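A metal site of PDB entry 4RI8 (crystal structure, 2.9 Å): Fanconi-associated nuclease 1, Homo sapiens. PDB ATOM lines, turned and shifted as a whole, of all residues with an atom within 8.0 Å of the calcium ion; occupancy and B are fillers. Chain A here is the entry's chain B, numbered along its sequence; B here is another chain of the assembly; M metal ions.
The side-chain amino group (NZ) of Lys 611 is in salt-bridge range of OP2 of DG 4 of chain B (3.7 Å).
O of Asp 594 is in hydrogen-bond range of N of Glu 468, at 2.8 Å.
The backbone NH of Asp 594 lies within hydrogen-bond range of the backbone carbonyl oxygen of Val 608.
The side-chain amide nitrogen (NE2) of Gln 621 is in hydrogen-bond range of the side-chain carboxylate (OE1) of Glu 609.
The side-chain carboxylate of Glu 449 lies within salt-bridge range of the side-chain amino group of Lys 428, 3.0 Å away.
The side-chain amino group of Lys 611 lies within salt-bridge range of the side-chain carboxylate of Asp 615 (3.1 Å).
The side-chain amide nitrogen (NE2) of Gln 621 lies close to the side-chain amino group (NZ) of Lys 611, 3.1 Å away.
The backbone NH of Lys 611 sits at hydrogen-bond distance from the backbone carbonyl oxygen of Cys 638, 2.8 Å away.
Merely in contact with the calcium ion: Glu 449 and Lys 611.
The nearest printed residue that does not touch the calcium ion is Asp 615 (4.5 Å).
The calcium ion is bound by OP1 of DG 4 of chain B (2.3 Å), OD2 of Asp 594 (2.3 Å), OE2 of Glu 609 (2.3 Å) and O of Val 610 (2.3 Å).
Slightly farther from the calcium ion lies OD1 of Asp 594 (3.1 Å).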
ATOM      1  N   LYS A 428       9.197  -4.395  34.965  1.00  0.00           N
ATOM      2  CA  LYS A 428       7.975  -5.106  34.610  1.00  0.00           C
ATOM      3  C   LYS A 428       6.737  -4.218  34.760  1.00  0.00           C
ATOM      4  O   LYS A 428       6.612  -3.494  35.748  1.00  0.00           O
ATOM      5  CB  LYS A 428       7.829  -6.387  35.436  1.00  0.00           C
ATOM      6  CG  LYS A 428       7.050  -7.479  34.717  1.00  0.00           C
ATOM      7  CD  LYS A 428       6.395  -8.464  35.673  1.00  0.00           C
ATOM      8  CE  LYS A 428       5.376  -9.323  34.923  1.00  0.00           C
ATOM      9  NZ  LYS A 428       4.629 -10.319  35.749  1.00  0.00           N
ATOM     10  N   VAL A 448       0.276  -7.748  35.016  1.00  0.00           N
ATOM     11  CA  VAL A 448      -0.580  -7.992  33.854  1.00  0.00           C
ATOM     12  C   VAL A 448      -1.380  -9.276  34.047  1.00  0.00           C
ATOM     13  O   VAL A 448      -2.610  -9.289  33.887  1.00  0.00           O
ATOM     14  CB  VAL A 448       0.260  -8.157  32.569  1.00  0.00           C
ATOM     15  CG1 VAL A 448      -0.639  -8.189  31.337  1.00  0.00           C
ATOM     16  CG2 VAL A 448       1.294  -7.048  32.451  1.00  0.00           C
ATOM     17  N   GLU A 449      -0.659 -10.334  34.394  1.00  0.00           N
ATOM     18  CA  GLU A 449      -1.236 -11.653  34.585  1.00  0.00           C
ATOM     19  C   GLU A 449      -2.229 -11.706  35.765  1.00  0.00           C
ATOM     20  O   GLU A 449      -3.258 -12.398  35.674  1.00  0.00           O
ATOM     21  CB  GLU A 449      -0.132 -12.712  34.733  1.00  0.00           C
ATOM     22  CG  GLU A 449       0.660 -12.999  33.441  1.00  0.00           C
ATOM     23  CD  GLU A 449       1.953 -12.194  33.308  1.00  0.00           C
ATOM     24  OE1 GLU A 449       2.350 -11.464  34.249  1.00  0.00           O
ATOM     25  OE2 GLU A 449       2.580 -12.308  32.226  1.00  0.00           O
ATOM     26  N   HIS A 466      -1.285 -18.494  38.318  1.00  0.00           N
ATOM     27  CA  HIS A 466      -0.253 -17.947  37.448  1.00  0.00           C
ATOM     28  C   HIS A 466       1.030 -18.753  37.667  1.00  0.00           C
ATOM     29  O   HIS A 466       1.813 -18.445  38.561  1.00  0.00           O
ATOM     30  CB  HIS A 466      -0.042 -16.437  37.731  1.00  0.00           C
ATOM     31  CG  HIS A 466       1.096 -15.822  36.953  1.00  0.00           C
ATOM     32  ND1 HIS A 466       1.469 -16.262  35.704  1.00  0.00           N
ATOM     33  CD2 HIS A 466       1.918 -14.794  37.255  1.00  0.00           C
ATOM     34  CE1 HIS A 466       2.495 -15.545  35.269  1.00  0.00           C
ATOM     35  NE2 HIS A 466       2.781 -14.644  36.195  1.00  0.00           N
ATOM     36  N   GLU A 468       2.810 -20.381  34.738  1.00  0.00           N
ATOM     37  CA  GLU A 468       3.466 -20.649  33.473  1.00  0.00           C
ATOM     38  C   GLU A 468       3.631 -22.159  33.311  1.00  0.00           C
ATOM     39  O   GLU A 468       2.689 -22.914  33.526  1.00  0.00           O
ATOM     40  CB  GLU A 468       4.802 -19.883  33.325  1.00  0.00           C
ATOM     41  CG  GLU A 468       4.892 -18.569  34.099  1.00  0.00           C
ATOM     42  CD  GLU A 468       5.336 -17.380  33.249  1.00  0.00           C
ATOM     43  OE1 GLU A 468       6.346 -17.526  32.522  1.00  0.00           O
ATOM     44  OE2 GLU A 468       4.686 -16.311  33.314  1.00  0.00           O
ATOM     45  N   LEU A 592       4.444 -22.898  27.692  1.00  0.00           N
ATOM     46  CA  LEU A 592       3.094 -23.173  28.157  1.00  0.00           C
ATOM     47  C   LEU A 592       2.478 -21.881  28.651  1.00  0.00           C
ATOM     48  O   LEU A 592       3.194 -20.976  29.060  1.00  0.00           O
ATOM     49  CB  LEU A 592       3.108 -24.221  29.251  1.00  0.00           C
ATOM     50  CG  LEU A 592       3.388 -25.645  28.787  1.00  0.00           C
ATOM     51  CD1 LEU A 592       3.922 -26.450  29.963  1.00  0.00           C
ATOM     52  CD2 LEU A 592       2.139 -26.274  28.196  1.00  0.00           C
ATOM     53  N   PRO A 593       1.143 -21.762  28.578  1.00  0.00           N
ATOM     54  CA  PRO A 593       0.381 -20.574  28.974  1.00  0.00           C
ATOM     55  C   PRO A 593       0.618 -20.091  30.400  1.00  0.00           C
ATOM     56  O   PRO A 593       0.788 -20.906  31.304  1.00  0.00           O
ATOM     57  CB  PRO A 593      -1.080 -21.032  28.847  1.00  0.00           C
ATOM     58  CG  PRO A 593      -1.063 -22.303  28.096  1.00  0.00           C
ATOM     59  CD  PRO A 593       0.333 -22.706  27.786  1.00  0.00           C
ATOM     60  N   ASP A 594       0.611 -18.776  30.602  1.00  0.00           N
ATOM     61  CA  ASP A 594       0.884 -18.192  31.912  1.00  0.00           C
ATOM     62  C   ASP A 594      -0.025 -18.783  32.981  1.00  0.00           C
ATOM     63  O   ASP A 594       0.434 -19.111  34.078  1.00  0.00           O
ATOM     64  CB  ASP A 594       0.717 -16.658  31.883  1.00  0.00           C
ATOM     65  CG  ASP A 594       1.741 -15.961  30.980  1.00  0.00           C
ATOM     66  OD1 ASP A 594       2.961 -15.987  31.277  1.00  0.00           O
ATOM     67  OD2 ASP A 594       1.316 -15.354  29.974  1.00  0.00           O
ATOM     68  N   LEU A 595      -1.292 -18.963  32.612  1.00  0.00           N
ATOM     69  CA  LEU A 595      -2.389 -19.209  33.555  1.00  0.00           C
ATOM     70  C   LEU A 595      -3.138 -20.529  33.336  1.00  0.00           C
ATOM     71  O   LEU A 595      -3.256 -21.007  32.197  1.00  0.00           O
ATOM     72  CB  LEU A 595      -3.428 -18.082  33.443  1.00  0.00           C
ATOM     73  CG  LEU A 595      -3.423 -16.838  34.316  1.00  0.00           C
ATOM     74  CD1 LEU A 595      -2.033 -16.243  34.507  1.00  0.00           C
ATOM     75  CD2 LEU A 595      -4.365 -15.828  33.696  1.00  0.00           C
ATOM     76  N   VAL A 608      -4.769 -20.075  29.638  1.00  0.00           N
ATOM     77  CA  VAL A 608      -4.769 -18.689  29.172  1.00  0.00           C
ATOM     78  C   VAL A 608      -3.378 -18.050  29.147  1.00  0.00           C
ATOM     79  O   VAL A 608      -2.749 -17.891  30.210  1.00  0.00           O
ATOM     80  CB  VAL A 608      -5.720 -17.828  30.055  1.00  0.00           C
ATOM     81  CG1 VAL A 608      -5.740 -16.384  29.582  1.00  0.00           C
ATOM     82  CG2 VAL A 608      -7.127 -18.413  30.052  1.00  0.00           C
ATOM     83  N   GLU A 609      -2.903 -17.691  27.952  1.00  0.00           N
ATOM     84  CA  GLU A 609      -1.671 -16.889  27.823  1.00  0.00           C
ATOM     85  C   GLU A 609      -2.020 -15.410  27.867  1.00  0.00           C
ATOM     86  O   GLU A 609      -2.770 -14.920  27.017  1.00  0.00           O
ATOM     87  CB  GLU A 609      -0.882 -17.223  26.552  1.00  0.00           C
ATOM     88  CG  GLU A 609       0.264 -16.249  26.238  1.00  0.00           C
ATOM     89  CD  GLU A 609       1.408 -16.234  27.249  1.00  0.00           C
ATOM     90  OE1 GLU A 609       1.855 -17.323  27.674  1.00  0.00           O
ATOM     91  OE2 GLU A 609       1.907 -15.149  27.608  1.00  0.00           O
ATOM     92  N   VAL A 610      -1.457 -14.715  28.847  1.00  0.00           N
ATOM     93  CA  VAL A 610      -1.654 -13.281  29.021  1.00  0.00           C
ATOM     94  C   VAL A 610      -0.558 -12.507  28.309  1.00  0.00           C
ATOM     95  O   VAL A 610       0.651 -12.697  28.561  1.00  0.00           O
ATOM     96  CB  VAL A 610      -1.728 -12.871  30.512  1.00  0.00           C
ATOM     97  CG1 VAL A 610      -2.114 -11.411  30.662  1.00  0.00           C
ATOM     98  CG2 VAL A 610      -2.717 -13.754  31.256  1.00  0.00           C
ATOM     99  N   LYS A 611      -1.011 -11.644  27.401  1.00  0.00           N
ATOM    100  CA  LYS A 611      -0.159 -10.829  26.560  1.00  0.00           C
ATOM    101  C   LYS A 611      -0.462  -9.373  26.838  1.00  0.00           C
ATOM    102  O   LYS A 611      -1.574  -8.894  26.593  1.00  0.00           O
ATOM    103  CB  LYS A 611      -0.442 -11.134  25.086  1.00  0.00           C
ATOM    104  CG  LYS A 611       0.070 -12.492  24.624  1.00  0.00           C
ATOM    105  CD  LYS A 611       1.577 -12.460  24.480  1.00  0.00           C
ATOM    106  CE  LYS A 611       2.197 -13.839  24.581  1.00  0.00           C
ATOM    107  NZ  LYS A 611       3.244 -13.826  25.628  1.00  0.00           N
ATOM    108  N   GLY A 612       0.531  -8.651  27.371  1.00  0.00           N
ATOM    109  CA  GLY A 612       0.372  -7.216  27.637  1.00  0.00           C
ATOM    110  C   GLY A 612       0.259  -6.419  26.347  1.00  0.00           C
ATOM    111  O   GLY A 612       0.258  -7.000  25.250  1.00  0.00           O
ATOM    112  N   ASP A 615       3.481  -7.145  23.845  1.00  0.00           N
ATOM    113  CA  ASP A 615       3.930  -8.445  23.319  1.00  0.00           C
ATOM    114  C   ASP A 615       2.909  -9.320  22.580  1.00  0.00           C
ATOM    115  O   ASP A 615       1.703  -9.223  22.791  1.00  0.00           O
ATOM    116  CB  ASP A 615       4.745  -9.262  24.374  1.00  0.00           C
ATOM    117  CG  ASP A 615       3.920  -9.648  25.608  1.00  0.00           C
ATOM    118  OD1 ASP A 615       3.373  -8.750  26.281  1.00  0.00           O
ATOM    119  OD2 ASP A 615       3.867 -10.855  25.938  1.00  0.00           O
ATOM    120  N   ARG A 616       3.447 -10.152  21.685  1.00  0.00           N
ATOM    121  CA  ARG A 616       2.690 -11.138  20.944  1.00  0.00           C
ATOM    122  C   ARG A 616       3.269 -12.526  21.255  1.00  0.00           C
ATOM    123  O   ARG A 616       4.191 -12.651  22.071  1.00  0.00           O
ATOM    124  CB  ARG A 616       2.749 -10.841  19.430  1.00  0.00           C
ATOM    125  CG  ARG A 616       2.339  -9.409  19.065  1.00  0.00           C
ATOM    126  CD  ARG A 616       2.010  -9.226  17.584  1.00  0.00           C
ATOM    127  NE  ARG A 616       3.145  -8.757  16.773  1.00  0.00           N
ATOM    128  CZ  ARG A 616       3.992  -9.552  16.111  1.00  0.00           C
ATOM    129  NH1 ARG A 616       3.862 -10.870  16.149  1.00  0.00           N
ATOM    130  NH2 ARG A 616       4.979  -9.020  15.406  1.00  0.00           N
ATOM    131  N   LEU A 617       2.730 -13.557  20.617  1.00  0.00           N
ATOM    132  CA  LEU A 617       3.078 -14.945  20.916  1.00  0.00           C
ATOM    133  C   LEU A 617       4.428 -15.302  20.368  1.00  0.00           C
ATOM    134  O   LEU A 617       4.718 -15.027  19.204  1.00  0.00           O
ATOM    135  CB  LEU A 617       2.060 -15.905  20.301  1.00  0.00           C
ATOM    136  CG  LEU A 617       0.609 -15.907  20.742  1.00  0.00           C
ATOM    137  CD1 LEU A 617      -0.217 -16.737  19.778  1.00  0.00           C
ATOM    138  CD2 LEU A 617       0.474 -16.409  22.178  1.00  0.00           C
ATOM    139  N   GLN A 621       5.137 -20.743  22.210  1.00  0.00           N
ATOM    140  CA  GLN A 621       3.794 -20.487  22.720  1.00  0.00           C
ATOM    141  C   GLN A 621       2.652 -20.963  21.802  1.00  0.00           C
ATOM    142  O   GLN A 621       1.683 -21.581  22.262  1.00  0.00           O
ATOM    143  CB  GLN A 621       3.635 -19.020  23.049  1.00  0.00           C
ATOM    144  CG  GLN A 621       4.059 -18.691  24.453  1.00  0.00           C
ATOM    145  CD  GLN A 621       4.304 -17.222  24.647  1.00  0.00           C
ATOM    146  OE1 GLN A 621       4.608 -16.494  23.695  1.00  0.00           O
ATOM    147  NE2 GLN A 621       4.186 -16.755  25.880  1.00  0.00           N
ATOM    148  N   CYS A 638      -5.222 -13.801  26.131  1.00  0.00           N
ATOM    149  CA  CYS A 638      -5.855 -12.661  26.755  1.00  0.00           C
ATOM    150  C   CYS A 638      -4.914 -11.489  26.576  1.00  0.00           C
ATOM    151  O   CYS A 638      -3.828 -11.475  27.158  1.00  0.00           O
ATOM    152  CB  CYS A 638      -6.102 -12.946  28.242  1.00  0.00           C
ATOM    153  SG  CYS A 638      -6.938 -11.647  29.191  1.00  0.00           S
ATOM    154  P    DG B   3       9.289 -19.527  28.261  1.00  0.00           P
ATOM    155  OP1  DG B   3       8.435 -20.628  28.798  1.00  0.00           O
ATOM    156  OP2  DG B   3       9.586 -19.474  26.797  1.00  0.00           O
ATOM    157  O5'  DG B   3       8.628 -18.143  28.706  1.00  0.00           O
ATOM    158  C5'  DG B   3       9.014 -17.483  29.931  1.00  0.00           C
ATOM    159  C4'  DG B   3       9.175 -15.994  29.738  1.00  0.00           C
ATOM    160  O4'  DG B   3      10.555 -15.658  29.469  1.00  0.00           O
ATOM    161  C3'  DG B   3       8.366 -15.377  28.590  1.00  0.00           C
ATOM    162  O3'  DG B   3       7.229 -14.731  29.176  1.00  0.00           O
ATOM    163  C2'  DG B   3       9.347 -14.437  27.891  1.00  0.00           C
ATOM    164  C1'  DG B   3      10.555 -14.404  28.812  1.00  0.00           C
ATOM    165  N9   DG B   3      11.852 -14.243  28.160  1.00  0.00           N
ATOM    166  C8   DG B   3      12.318 -14.897  27.053  1.00  0.00           C
ATOM    167  N7   DG B   3      13.528 -14.540  26.705  1.00  0.00           N
ATOM    168  C5   DG B   3      13.881 -13.574  27.645  1.00  0.00           C
ATOM    169  C6   DG B   3      15.075 -12.818  27.779  1.00  0.00           C
ATOM    170  O6   DG B   3      16.089 -12.861  27.078  1.00  0.00           O
ATOM    171  N1   DG B   3      15.013 -11.966  28.870  1.00  0.00           N
ATOM    172  C2   DG B   3      13.944 -11.838  29.724  1.00  0.00           C
ATOM    173  N2   DG B   3      14.077 -10.955  30.726  1.00  0.00           N
ATOM    174  N3   DG B   3      12.828 -12.536  29.611  1.00  0.00           N
ATOM    175  C4   DG B   3      12.865 -13.388  28.553  1.00  0.00           C
ATOM    176  P    DG B   4       6.337 -13.684  28.353  1.00  0.00           P
ATOM    177  OP1  DG B   4       4.910 -13.910  28.722  1.00  0.00           O
ATOM    178  OP2  DG B   4       6.741 -13.726  26.925  1.00  0.00           O
ATOM    179  O5'  DG B   4       6.769 -12.284  28.997  1.00  0.00           O
ATOM    180  C5'  DG B   4       6.919 -12.157  30.427  1.00  0.00           C
ATOM    181  C4'  DG B   4       7.390 -10.775  30.805  1.00  0.00           C
ATOM    182  O4'  DG B   4       8.782 -10.607  30.471  1.00  0.00           O
ATOM    183  C3'  DG B   4       6.645  -9.620  30.138  1.00  0.00           C
ATOM    184  O3'  DG B   4       6.415  -8.606  31.125  1.00  0.00           O
ATOM    185  C2'  DG B   4       7.591  -9.165  29.036  1.00  0.00           C
ATOM    186  C1'  DG B   4       8.969  -9.515  29.589  1.00  0.00           C
ATOM    187  N9   DG B   4       9.936  -9.927  28.562  1.00  0.00           N
ATOM    188  C8   DG B   4       9.739 -10.881  27.588  1.00  0.00           C
ATOM    189  N7   DG B   4      10.793 -11.049  26.835  1.00  0.00           N
ATOM    190  C5   DG B   4      11.728 -10.173  27.336  1.00  0.00           C
ATOM    191  C6   DG B   4      13.061  -9.899  26.919  1.00  0.00           C
ATOM    192  O6   DG B   4      13.700 -10.420  25.992  1.00  0.00           O
ATOM    193  N1   DG B   4      13.659  -8.919  27.702  1.00  0.00           N
ATOM    194  C2   DG B   4      13.060  -8.275  28.758  1.00  0.00           C
ATOM    195  N2   DG B   4      13.801  -7.366  29.403  1.00  0.00           N
ATOM    196  N3   DG B   4      11.819  -8.515  29.166  1.00  0.00           N
ATOM    197  C4   DG B   4      11.215  -9.472  28.415  1.00  0.00           C
ATOM    198  P    DC B   5       5.284  -7.502  30.879  1.00  0.00           P
ATOM    199  OP1  DC B   5       4.632  -7.218  32.183  1.00  0.00           O
ATOM    200  OP2  DC B   5       4.460  -7.917  29.721  1.00  0.00           O
ATOM    201  O5'  DC B   5       6.150  -6.221  30.513  1.00  0.00           O
ATOM    202  C5'  DC B   5       7.363  -5.925  31.236  1.00  0.00           C
ATOM    203  C4'  DC B   5       8.210  -4.938  30.481  1.00  0.00           C
ATOM    204  O4'  DC B   5       9.187  -5.640  29.687  1.00  0.00           O
ATOM    205  C3'  DC B   5       7.432  -4.027  29.513  1.00  0.00           C
ATOM    206  O3'  DC B   5       7.778  -2.648  29.713  1.00  0.00           O
ATOM    207  C2'  DC B   5       7.913  -4.472  28.148  1.00  0.00           C
ATOM    208  C1'  DC B   5       9.310  -4.958  28.455  1.00  0.00           C
ATOM    209  N1   DC B   5       9.854  -5.887  27.456  1.00  0.00           N
ATOM    210  C2   DC B   5      11.228  -5.853  27.191  1.00  0.00           C
ATOM    211  O2   DC B   5      11.948  -5.099  27.857  1.00  0.00           O
ATOM    212  N3   DC B   5      11.725  -6.667  26.228  1.00  0.00           N
ATOM    213  C4   DC B   5      10.907  -7.472  25.546  1.00  0.00           C
ATOM    214  N4   DC B   5      11.450  -8.269  24.614  1.00  0.00           N
ATOM    215  C5   DC B   5       9.508  -7.501  25.779  1.00  0.00           C
ATOM    216  C6   DC B   5       9.023  -6.691  26.722  1.00  0.00           C
HETATM  217 CA    CA M   1       2.673 -13.661  29.194  1.00  0.00          CA
